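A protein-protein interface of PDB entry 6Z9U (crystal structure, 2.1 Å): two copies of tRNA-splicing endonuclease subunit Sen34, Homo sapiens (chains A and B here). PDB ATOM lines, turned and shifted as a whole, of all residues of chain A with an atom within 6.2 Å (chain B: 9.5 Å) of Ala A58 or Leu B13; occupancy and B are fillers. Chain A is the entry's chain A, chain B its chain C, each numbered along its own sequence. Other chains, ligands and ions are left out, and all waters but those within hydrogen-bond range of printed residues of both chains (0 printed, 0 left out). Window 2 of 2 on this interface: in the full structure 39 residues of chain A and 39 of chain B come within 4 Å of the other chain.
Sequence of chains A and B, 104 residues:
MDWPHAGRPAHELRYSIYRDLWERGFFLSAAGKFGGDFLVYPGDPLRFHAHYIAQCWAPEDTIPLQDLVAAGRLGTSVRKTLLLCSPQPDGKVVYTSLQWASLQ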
ATOM      1  N   CYS A  56     -23.117   2.536 -14.366  1.00  0.00           N
ATOM      2  CA  CYS A  56     -23.975   3.655 -14.724  1.00  0.00           C
ATOM      3  C   CYS A  56     -25.430   3.238 -14.607  1.00  0.00           C
ATOM      4  O   CYS A  56     -25.846   2.234 -15.199  1.00  0.00           O
ATOM      5  CB  CYS A  56     -23.686   4.121 -16.151  1.00  0.00           C
ATOM      6  SG  CYS A  56     -22.000   4.697 -16.388  1.00  0.00           S
ATOM      7  N   TRP A  57     -26.204   4.012 -13.857  1.00  0.00           N
ATOM      8  CA  TRP A  57     -27.603   3.687 -13.623  1.00  0.00           C
ATOM      9  C   TRP A  57     -28.446   4.931 -13.787  1.00  0.00           C
ATOM     10  O   TRP A  57     -28.148   5.967 -13.190  1.00  0.00           O
ATOM     11  CB  TRP A  57     -27.801   3.102 -12.228  1.00  0.00           C
ATOM     12  CG  TRP A  57     -27.329   1.707 -12.134  1.00  0.00           C
ATOM     13  CD1 TRP A  57     -26.183   1.261 -11.537  1.00  0.00           C
ATOM     14  CD2 TRP A  57     -27.983   0.552 -12.677  1.00  0.00           C
ATOM     15  NE1 TRP A  57     -26.104  -0.115 -11.652  1.00  0.00           N
ATOM     16  CE2 TRP A  57     -27.183  -0.567 -12.365  1.00  0.00           C
ATOM     17  CE3 TRP A  57     -29.164   0.360 -13.409  1.00  0.00           C
ATOM     18  CZ2 TRP A  57     -27.529  -1.868 -12.758  1.00  0.00           C
ATOM     19  CZ3 TRP A  57     -29.501  -0.926 -13.805  1.00  0.00           C
ATOM     20  CH2 TRP A  57     -28.690  -2.026 -13.473  1.00  0.00           C
ATOM     21  N   ALA A  58     -29.492   4.833 -14.590  1.00  0.00           N
ATOM     22  CA  ALA A  58     -30.517   5.854 -14.525  1.00  0.00           C
ATOM     23  C   ALA A  58     -31.130   5.813 -13.127  1.00  0.00           C
ATOM     24  O   ALA A  58     -31.294   4.725 -12.557  1.00  0.00           O
ATOM     25  CB  ALA A  58     -31.585   5.635 -15.598  1.00  0.00           C
ATOM     26  N   PRO A  59     -31.435   6.968 -12.530  1.00  0.00           N
ATOM     27  CA  PRO A  59     -31.803   6.973 -11.104  1.00  0.00           C
ATOM     28  C   PRO A  59     -33.011   6.110 -10.784  1.00  0.00           C
ATOM     29  O   PRO A  59     -33.083   5.567  -9.676  1.00  0.00           O
ATOM     30  CB  PRO A  59     -32.078   8.456 -10.818  1.00  0.00           C
ATOM     31  CG  PRO A  59     -31.363   9.193 -11.874  1.00  0.00           C
ATOM     32  CD  PRO A  59     -31.358   8.327 -13.090  1.00  0.00           C
ATOM     33  N   GLU A  60     -33.940   5.939 -11.729  1.00  0.00           N
ATOM     34  CA  GLU A  60     -35.193   5.229 -11.480  1.00  0.00           C
ATOM     35  C   GLU A  60     -35.155   3.752 -11.859  1.00  0.00           C
ATOM     36  O   GLU A  60     -36.058   3.007 -11.466  1.00  0.00           O
ATOM     37  CB  GLU A  60     -36.346   5.911 -12.232  1.00  0.00           C
ATOM     38  CG  GLU A  60     -37.047   7.001 -11.435  1.00  0.00           C
ATOM     39  CD  GLU A  60     -37.667   6.469 -10.144  1.00  0.00           C
ATOM     40  OE1 GLU A  60     -37.319   6.972  -9.052  1.00  0.00           O
ATOM     41  OE2 GLU A  60     -38.495   5.534 -10.223  1.00  0.00           O
ATOM     42  N   ASP A  61     -34.146   3.310 -12.607  1.00  0.00           N
ATOM     43  CA  ASP A  61     -34.094   1.919 -13.041  1.00  0.00           C
ATOM     44  C   ASP A  61     -33.833   0.999 -11.861  1.00  0.00           C
ATOM     45  O   ASP A  61     -32.896   1.213 -11.087  1.00  0.00           O
ATOM     46  CB  ASP A  61     -33.005   1.730 -14.089  1.00  0.00           C
ATOM     47  CG  ASP A  61     -33.368   2.349 -15.399  1.00  0.00           C
ATOM     48  OD1 ASP A  61     -34.582   2.518 -15.652  1.00  0.00           O
ATOM     49  OD2 ASP A  61     -32.443   2.662 -16.175  1.00  0.00           O
ATOM     50  N   THR A  62     -34.654  -0.034 -11.723  1.00  0.00           N
ATOM     51  CA  THR A  62     -34.485  -0.938 -10.600  1.00  0.00           C
ATOM     52  C   THR A  62     -33.316  -1.859 -10.896  1.00  0.00           C
ATOM     53  O   THR A  62     -33.248  -2.466 -11.968  1.00  0.00           O
ATOM     54  CB  THR A  62     -35.761  -1.744 -10.331  1.00  0.00           C
ATOM     55  OG1 THR A  62     -35.907  -2.771 -11.318  1.00  0.00           O
ATOM     56  CG2 THR A  62     -36.982  -0.840 -10.366  1.00  0.00           C
ATOM     57  N   CYS A  85     -23.461   4.823  -9.795  1.00  0.00           N
ATOM     58  CA  CYS A  85     -23.398   6.210 -10.249  1.00  0.00           C
ATOM     59  C   CYS A  85     -24.675   6.547 -10.995  1.00  0.00           C
ATOM     60  O   CYS A  85     -25.113   5.776 -11.858  1.00  0.00           O
ATOM     61  CB  CYS A  85     -22.178   6.469 -11.205  1.00  0.00           C
ATOM     62  SG  CYS A  85     -20.703   5.502 -10.823  1.00  0.00           S
ATOM     63  N   SER A  86     -25.263   7.706 -10.673  1.00  0.00           N
ATOM     64  CA  SER A  86     -26.505   8.123 -11.303  1.00  0.00           C
ATOM     65  C   SER A  86     -26.530   9.638 -11.390  1.00  0.00           C
ATOM     66  O   SER A  86     -26.331  10.299 -10.360  1.00  0.00           O
ATOM     67  CB  SER A  86     -27.729   7.631 -10.523  1.00  0.00           C
ATOM     68  OG  SER A  86     -27.751   6.220 -10.545  1.00  0.00           O
ATOM     69  N   PRO A  87     -26.755  10.212 -12.571  1.00  0.00           N
ATOM     70  CA  PRO A  87     -26.910  11.668 -12.665  1.00  0.00           C
ATOM     71  C   PRO A  87     -28.328  12.100 -12.330  1.00  0.00           C
ATOM     72  O   PRO A  87     -29.307  11.456 -12.713  1.00  0.00           O
ATOM     73  CB  PRO A  87     -26.582  11.964 -14.130  1.00  0.00           C
ATOM     74  CG  PRO A  87     -27.004  10.728 -14.835  1.00  0.00           C
ATOM     75  CD  PRO A  87     -26.697   9.581 -13.901  1.00  0.00           C
ATOM     76  N   PRO B   9     -29.630   9.445 -25.009  1.00  0.00           N
ATOM     77  CA  PRO B   9     -29.999   8.061 -24.700  1.00  0.00           C
ATOM     78  C   PRO B   9     -29.623   7.661 -23.263  1.00  0.00           C
ATOM     79  O   PRO B   9     -29.435   8.532 -22.414  1.00  0.00           O
ATOM     80  CB  PRO B   9     -29.189   7.244 -25.723  1.00  0.00           C
ATOM     81  CG  PRO B   9     -28.468   8.267 -26.620  1.00  0.00           C
ATOM     82  CD  PRO B   9     -29.131   9.584 -26.387  1.00  0.00           C
ATOM     83  N   ALA B  10     -29.512   6.355 -23.001  1.00  0.00           N
ATOM     84  CA  ALA B  10     -28.762   5.848 -21.853  1.00  0.00           C
ATOM     85  C   ALA B  10     -27.260   5.994 -22.057  1.00  0.00           C
ATOM     86  O   ALA B  10     -26.452   5.517 -21.256  1.00  0.00           O
ATOM     87  CB  ALA B  10     -29.118   4.380 -21.597  1.00  0.00           C
ATOM     88  N   HIS B  11     -26.904   6.648 -23.149  1.00  0.00           N
ATOM     89  CA  HIS B  11     -25.551   6.873 -23.622  1.00  0.00           C
ATOM     90  C   HIS B  11     -25.065   8.268 -23.264  1.00  0.00           C
ATOM     91  O   HIS B  11     -23.855   8.484 -23.121  1.00  0.00           O
ATOM     92  CB  HIS B  11     -25.573   6.587 -25.133  1.00  0.00           C
ATOM     93  CG  HIS B  11     -24.528   7.269 -25.951  1.00  0.00           C
ATOM     94  ND1 HIS B  11     -23.435   6.603 -26.461  1.00  0.00           N
ATOM     95  CD2 HIS B  11     -24.464   8.530 -26.442  1.00  0.00           C
ATOM     96  CE1 HIS B  11     -22.724   7.436 -27.200  1.00  0.00           C
ATOM     97  NE2 HIS B  11     -23.320   8.614 -27.195  1.00  0.00           N
ATOM     98  N   GLU B  12     -26.005   9.204 -23.079  1.00  0.00           N
ATOM     99  CA  GLU B  12     -25.726  10.443 -22.361  1.00  0.00           C
ATOM    100  C   GLU B  12     -25.468  10.179 -20.886  1.00  0.00           C
ATOM    101  O   GLU B  12     -24.739  10.935 -20.235  1.00  0.00           O
ATOM    102  CB  GLU B  12     -26.902  11.411 -22.510  1.00  0.00           C
ATOM    103  CG  GLU B  12     -27.192  11.844 -23.938  1.00  0.00           C
ATOM    104  CD  GLU B  12     -26.215  12.892 -24.443  1.00  0.00           C
ATOM    105  OE1 GLU B  12     -25.388  13.375 -23.638  1.00  0.00           O
ATOM    106  OE2 GLU B  12     -26.280  13.236 -25.643  1.00  0.00           O
ATOM    107  N   LEU B  13     -26.092   9.134 -20.338  1.00  0.00           N
ATOM    108  CA  LEU B  13     -25.853   8.748 -18.956  1.00  0.00           C
ATOM    109  C   LEU B  13     -24.364   8.569 -18.683  1.00  0.00           C
ATOM    110  O   LEU B  13     -23.824   9.121 -17.717  1.00  0.00           O
ATOM    111  CB  LEU B  13     -26.597   7.451 -18.654  1.00  0.00           C
ATOM    112  CG  LEU B  13     -27.097   7.334 -17.242  1.00  0.00           C
ATOM    113  CD1 LEU B  13     -28.029   8.422 -17.039  1.00  0.00           C
ATOM    114  CD2 LEU B  13     -27.779   6.073 -17.056  1.00  0.00           C
ATOM    115  N   ARG B  14     -23.683   7.793 -19.534  1.00  0.00           N
ATOM    116  CA  ARG B  14     -22.287   7.464 -19.271  1.00  0.00           C
ATOM    117  C   ARG B  14     -21.391   8.687 -19.396  1.00  0.00           C
ATOM    118  O   ARG B  14     -20.421   8.826 -18.639  1.00  0.00           O
ATOM    119  CB  ARG B  14     -21.824   6.359 -20.218  1.00  0.00           C
ATOM    120  CG  ARG B  14     -22.692   5.125 -20.146  1.00  0.00           C
ATOM    121  CD  ARG B  14     -22.040   3.941 -20.828  1.00  0.00           C
ATOM    122  NE  ARG B  14     -20.890   3.445 -20.080  1.00  0.00           N
ATOM    123  CZ  ARG B  14     -20.898   2.339 -19.343  1.00  0.00           C
ATOM    124  NH1 ARG B  14     -22.000   1.605 -19.250  1.00  0.00           N
ATOM    125  NH2 ARG B  14     -19.797   1.962 -18.704  1.00  0.00           N
ATOM    126  N   TYR B  15     -21.711   9.581 -20.335  1.00  0.00           N
ATOM    127  CA  TYR B  15     -20.933  10.802 -20.531  1.00  0.00           C
ATOM    128  C   TYR B  15     -20.948  11.684 -19.292  1.00  0.00           C
ATOM    129  O   TYR B  15     -19.891  12.121 -18.815  1.00  0.00           O
ATOM    130  CB  TYR B  15     -21.482  11.572 -21.725  1.00  0.00           C
ATOM    131  CG  TYR B  15     -21.236  10.866 -23.021  1.00  0.00           C
ATOM    132  CD1 TYR B  15     -20.138  10.038 -23.164  1.00  0.00           C
ATOM    133  CD2 TYR B  15     -22.088  11.024 -24.105  1.00  0.00           C
ATOM    134  CE1 TYR B  15     -19.892   9.383 -24.337  1.00  0.00           C
ATOM    135  CE2 TYR B  15     -21.841  10.371 -25.297  1.00  0.00           C
ATOM    136  CZ  TYR B  15     -20.733   9.549 -25.401  1.00  0.00           C
ATOM    137  OH  TYR B  15     -20.438   8.882 -26.563  1.00  0.00           O
ATOM    138  N   SER B  16     -22.145  11.986 -18.778  1.00  0.00           N
ATOM    139  CA  SER B  16     -22.242  12.821 -17.587  1.00  0.00           C
ATOM    140  C   SER B  16     -21.424  12.236 -16.438  1.00  0.00           C
ATOM    141  O   SER B  16     -20.640  12.945 -15.794  1.00  0.00           O
ATOM    142  CB  SER B  16     -23.710  12.991 -17.190  1.00  0.00           C
ATOM    143  OG  SER B  16     -24.427  11.777 -17.337  1.00  0.00           O
ATOM    144  N   ILE B  17     -21.573  10.932 -16.185  1.00  0.00           N
ATOM    145  CA  ILE B  17     -20.805  10.285 -15.122  1.00  0.00           C
ATOM    146  C   ILE B  17     -19.303  10.381 -15.414  1.00  0.00           C
ATOM    147  O   ILE B  17     -18.518  10.857 -14.580  1.00  0.00           O
ATOM    148  CB  ILE B  17     -21.284   8.832 -14.943  1.00  0.00           C
ATOM    149  CG1 ILE B  17     -22.742   8.829 -14.428  1.00  0.00           C
ATOM    150  CG2 ILE B  17     -20.364   8.052 -13.999  1.00  0.00           C
ATOM    151  CD1 ILE B  17     -23.438   7.493 -14.487  1.00  0.00           C
ATOM    152  N   TYR B  18     -18.888   9.967 -16.620  1.00  0.00           N
ATOM    153  CA  TYR B  18     -17.466   9.997 -16.971  1.00  0.00           C
ATOM    154  C   TYR B  18     -16.879  11.389 -16.771  1.00  0.00           C
ATOM    155  O   TYR B  18     -15.764  11.546 -16.254  1.00  0.00           O
ATOM    156  CB  TYR B  18     -17.254   9.557 -18.432  1.00  0.00           C
ATOM    157  CG  TYR B  18     -17.421   8.077 -18.687  1.00  0.00           C
ATOM    158  CD1 TYR B  18     -17.893   7.221 -17.684  1.00  0.00           C
ATOM    159  CD2 TYR B  18     -17.112   7.526 -19.931  1.00  0.00           C
ATOM    160  CE1 TYR B  18     -18.046   5.868 -17.920  1.00  0.00           C
ATOM    161  CE2 TYR B  18     -17.268   6.168 -20.177  1.00  0.00           C
ATOM    162  CZ  TYR B  18     -17.735   5.341 -19.163  1.00  0.00           C
ATOM    163  OH  TYR B  18     -17.883   3.990 -19.400  1.00  0.00           O
ATOM    164  N   ARG B  19     -17.618  12.412 -17.185  1.00  0.00           N
ATOM    165  CA  ARG B  19     -17.100  13.762 -17.076  1.00  0.00           C
ATOM    166  C   ARG B  19     -16.981  14.169 -15.619  1.00  0.00           C
ATOM    167  O   ARG B  19     -15.953  14.713 -15.201  1.00  0.00           O
ATOM    168  CB  ARG B  19     -17.991  14.730 -17.843  1.00  0.00           C
ATOM    169  CG  ARG B  19     -17.265  15.996 -18.247  1.00  0.00           C
ATOM    170  CD  ARG B  19     -17.863  17.188 -17.555  1.00  0.00           C
ATOM    171  NE  ARG B  19     -19.309  17.210 -17.737  1.00  0.00           N
ATOM    172  CZ  ARG B  19     -20.113  18.107 -17.182  1.00  0.00           C
ATOM    173  NH1 ARG B  19     -19.606  19.056 -16.407  1.00  0.00           N
ATOM    174  NH2 ARG B  19     -21.421  18.055 -17.400  1.00  0.00           N
ATOM    175  N   ASP B  20     -18.025  13.897 -14.826  1.00  0.00           N
ATOM    176  CA  ASP B  20     -17.965  14.218 -13.409  1.00  0.00           C
ATOM    177  C   ASP B  20     -16.790  13.513 -12.742  1.00  0.00           C
ATOM    178  O   ASP B  20     -16.022  14.133 -12.001  1.00  0.00           O
ATOM    179  CB  ASP B  20     -19.284  13.841 -12.734  1.00  0.00           C
ATOM    180  CG  ASP B  20     -19.331  14.272 -11.293  1.00  0.00           C
ATOM    181  OD1 ASP B  20     -19.608  15.459 -11.060  1.00  0.00           O
ATOM    182  OD2 ASP B  20     -19.118  13.422 -10.399  1.00  0.00           O
ATOM    183  N   LEU B  21     -16.627  12.205 -13.004  1.00  0.00           N
ATOM    184  CA  LEU B  21     -15.498  11.486 -12.419  1.00  0.00           C
ATOM    185  C   LEU B  21     -14.167  12.113 -12.839  1.00  0.00           C
ATOM    186  O   LEU B  21     -13.257  12.272 -12.010  1.00  0.00           O
ATOM    187  CB  LEU B  21     -15.541  10.019 -12.821  1.00  0.00           C
ATOM    188  CG  LEU B  21     -16.618   9.232 -12.015  1.00  0.00           C
ATOM    189  CD1 LEU B  21     -16.755   7.845 -12.560  1.00  0.00           C
ATOM    190  CD2 LEU B  21     -16.303   9.183 -10.515  1.00  0.00           C
ATOM    191  N   PHE B  34     -20.020   0.238 -23.549  1.00  0.00           N
ATOM    192  CA  PHE B  34     -21.224   0.982 -23.172  1.00  0.00           C
ATOM    193  C   PHE B  34     -22.326  -0.045 -22.961  1.00  0.00           C
ATOM    194  O   PHE B  34     -22.996  -0.475 -23.897  1.00  0.00           O
ATOM    195  CB  PHE B  34     -21.594   2.012 -24.236  1.00  0.00           C
ATOM    196  CG  PHE B  34     -20.762   3.278 -24.190  1.00  0.00           C
ATOM    197  CD1 PHE B  34     -19.376   3.221 -24.174  1.00  0.00           C
ATOM    198  CD2 PHE B  34     -21.371   4.522 -24.183  1.00  0.00           C
ATOM    199  CE1 PHE B  34     -18.612   4.378 -24.132  1.00  0.00           C
ATOM    200  CE2 PHE B  34     -20.614   5.686 -24.140  1.00  0.00           C
ATOM    201  CZ  PHE B  34     -19.232   5.612 -24.117  1.00  0.00           C
ATOM    202  N   GLY B  35     -22.499  -0.451 -21.713  1.00  0.00           N
ATOM    203  CA  GLY B  35     -23.357  -1.568 -21.375  1.00  0.00           C
ATOM    204  C   GLY B  35     -22.704  -2.417 -20.307  1.00  0.00           C
ATOM    205  O   GLY B  35     -23.310  -3.349 -19.778  1.00  0.00           O
ATOM    206  N   PHE B  38     -17.171  -0.264 -15.672  1.00  0.00           N
ATOM    207  CA  PHE B  38     -15.919   0.385 -16.001  1.00  0.00           C
ATOM    208  C   PHE B  38     -15.133   0.526 -14.713  1.00  0.00           C
ATOM    209  O   PHE B  38     -15.631   0.220 -13.615  1.00  0.00           O
ATOM    210  CB  PHE B  38     -16.130   1.737 -16.705  1.00  0.00           C
ATOM    211  CG  PHE B  38     -16.943   2.744 -15.923  1.00  0.00           C
ATOM    212  CD1 PHE B  38     -16.340   3.888 -15.413  1.00  0.00           C
ATOM    213  CD2 PHE B  38     -18.315   2.577 -15.744  1.00  0.00           C
ATOM    214  CE1 PHE B  38     -17.069   4.808 -14.719  1.00  0.00           C
ATOM    215  CE2 PHE B  38     -19.060   3.506 -15.048  1.00  0.00           C
ATOM    216  CZ  PHE B  38     -18.443   4.619 -14.535  1.00  0.00           C
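The backbone NH (N) of Trp A57 lies within hydrogen-bond range of the backbone carbonyl oxygen (O) of Cys A85 (2.9 Å).
OG of Ser B16 lies within hydrogen-bond range of O of Glu B12 (3.0 Å).
The guanidinium group (NH2) of Arg B14 is in hydrogen-bond range of the side-chain hydroxyl (OH) of Tyr B18 (2.9 Å).
O of Leu B13 is in hydrogen-bond range of OG of Ser B16, 2.7 Å away.
The side-chain hydroxyl of Ser A86 is in hydrogen-bond range of the backbone carbonyl oxygen of Trp A57 (2.7 Å).
No position is printed for both chains.
Printed residues of chain A that touch a printed residue of chain B: Cys A56, Trp A57, Ala A58, Cys A85 and Pro A87.
Hydrophobic or aromatic side chains of chain A within 4 Å of the printed part of chain B: Pro A87.
Of the 16 printed residues of chain B, 5 touch a printed residue of chain A.
Among the printed residues, no Asp or Glu carboxylate lies within 4 Å of a Lys or Arg side-chain nitrogen of the other chain.
Leu B13 touches just these residues of chain A: Trp A57, Ala A58 and Pro A87.
No residue of chain B comes within 4 Å of Pro A59.
No residue of chain B comes within 4 Å of Asp A61.
Of the printed residues of chain A, Arg B14 touches Cys A56 (3.8 Å).
Printed residues of chain B within 4 Å of Trp A57: Leu B13 (3.5 Å).
Of the printed residues of chain B, Cys A56 touches Arg B14, Ile B17 and Phe B38.
Of the printed residues of chain B, Pro A87 touches Leu B13 (3.4 Å), Ser B16 (3.7 Å) and Ile B17 (3.9 Å).
Printed residues of chain B within 4 Å of Cys A85: Ile B17 (3.6 Å).
Thr A62 touches none of the printed residues of chain B.
Ala B10 touches none of the printed residues of chain A.
The nearest printed residue of chain B that does not touch Ala A58 is Ala B10 (6.6 Å).
The nearest residue of chain A that does not touch Leu B13 is Cys A56 (4.4 Å).
Among the printed residues, merely in contact across the chains: Cys A56 with Arg B14, Cys A56 with Ile B17, Cys A56 with Phe B38, Trp A57 with Leu B13, Ala A58 with Leu B13, Cys A85 with Ile B17, Pro A87 with Leu B13, Pro A87 with Ser B16 and Pro A87 with Ile B17.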
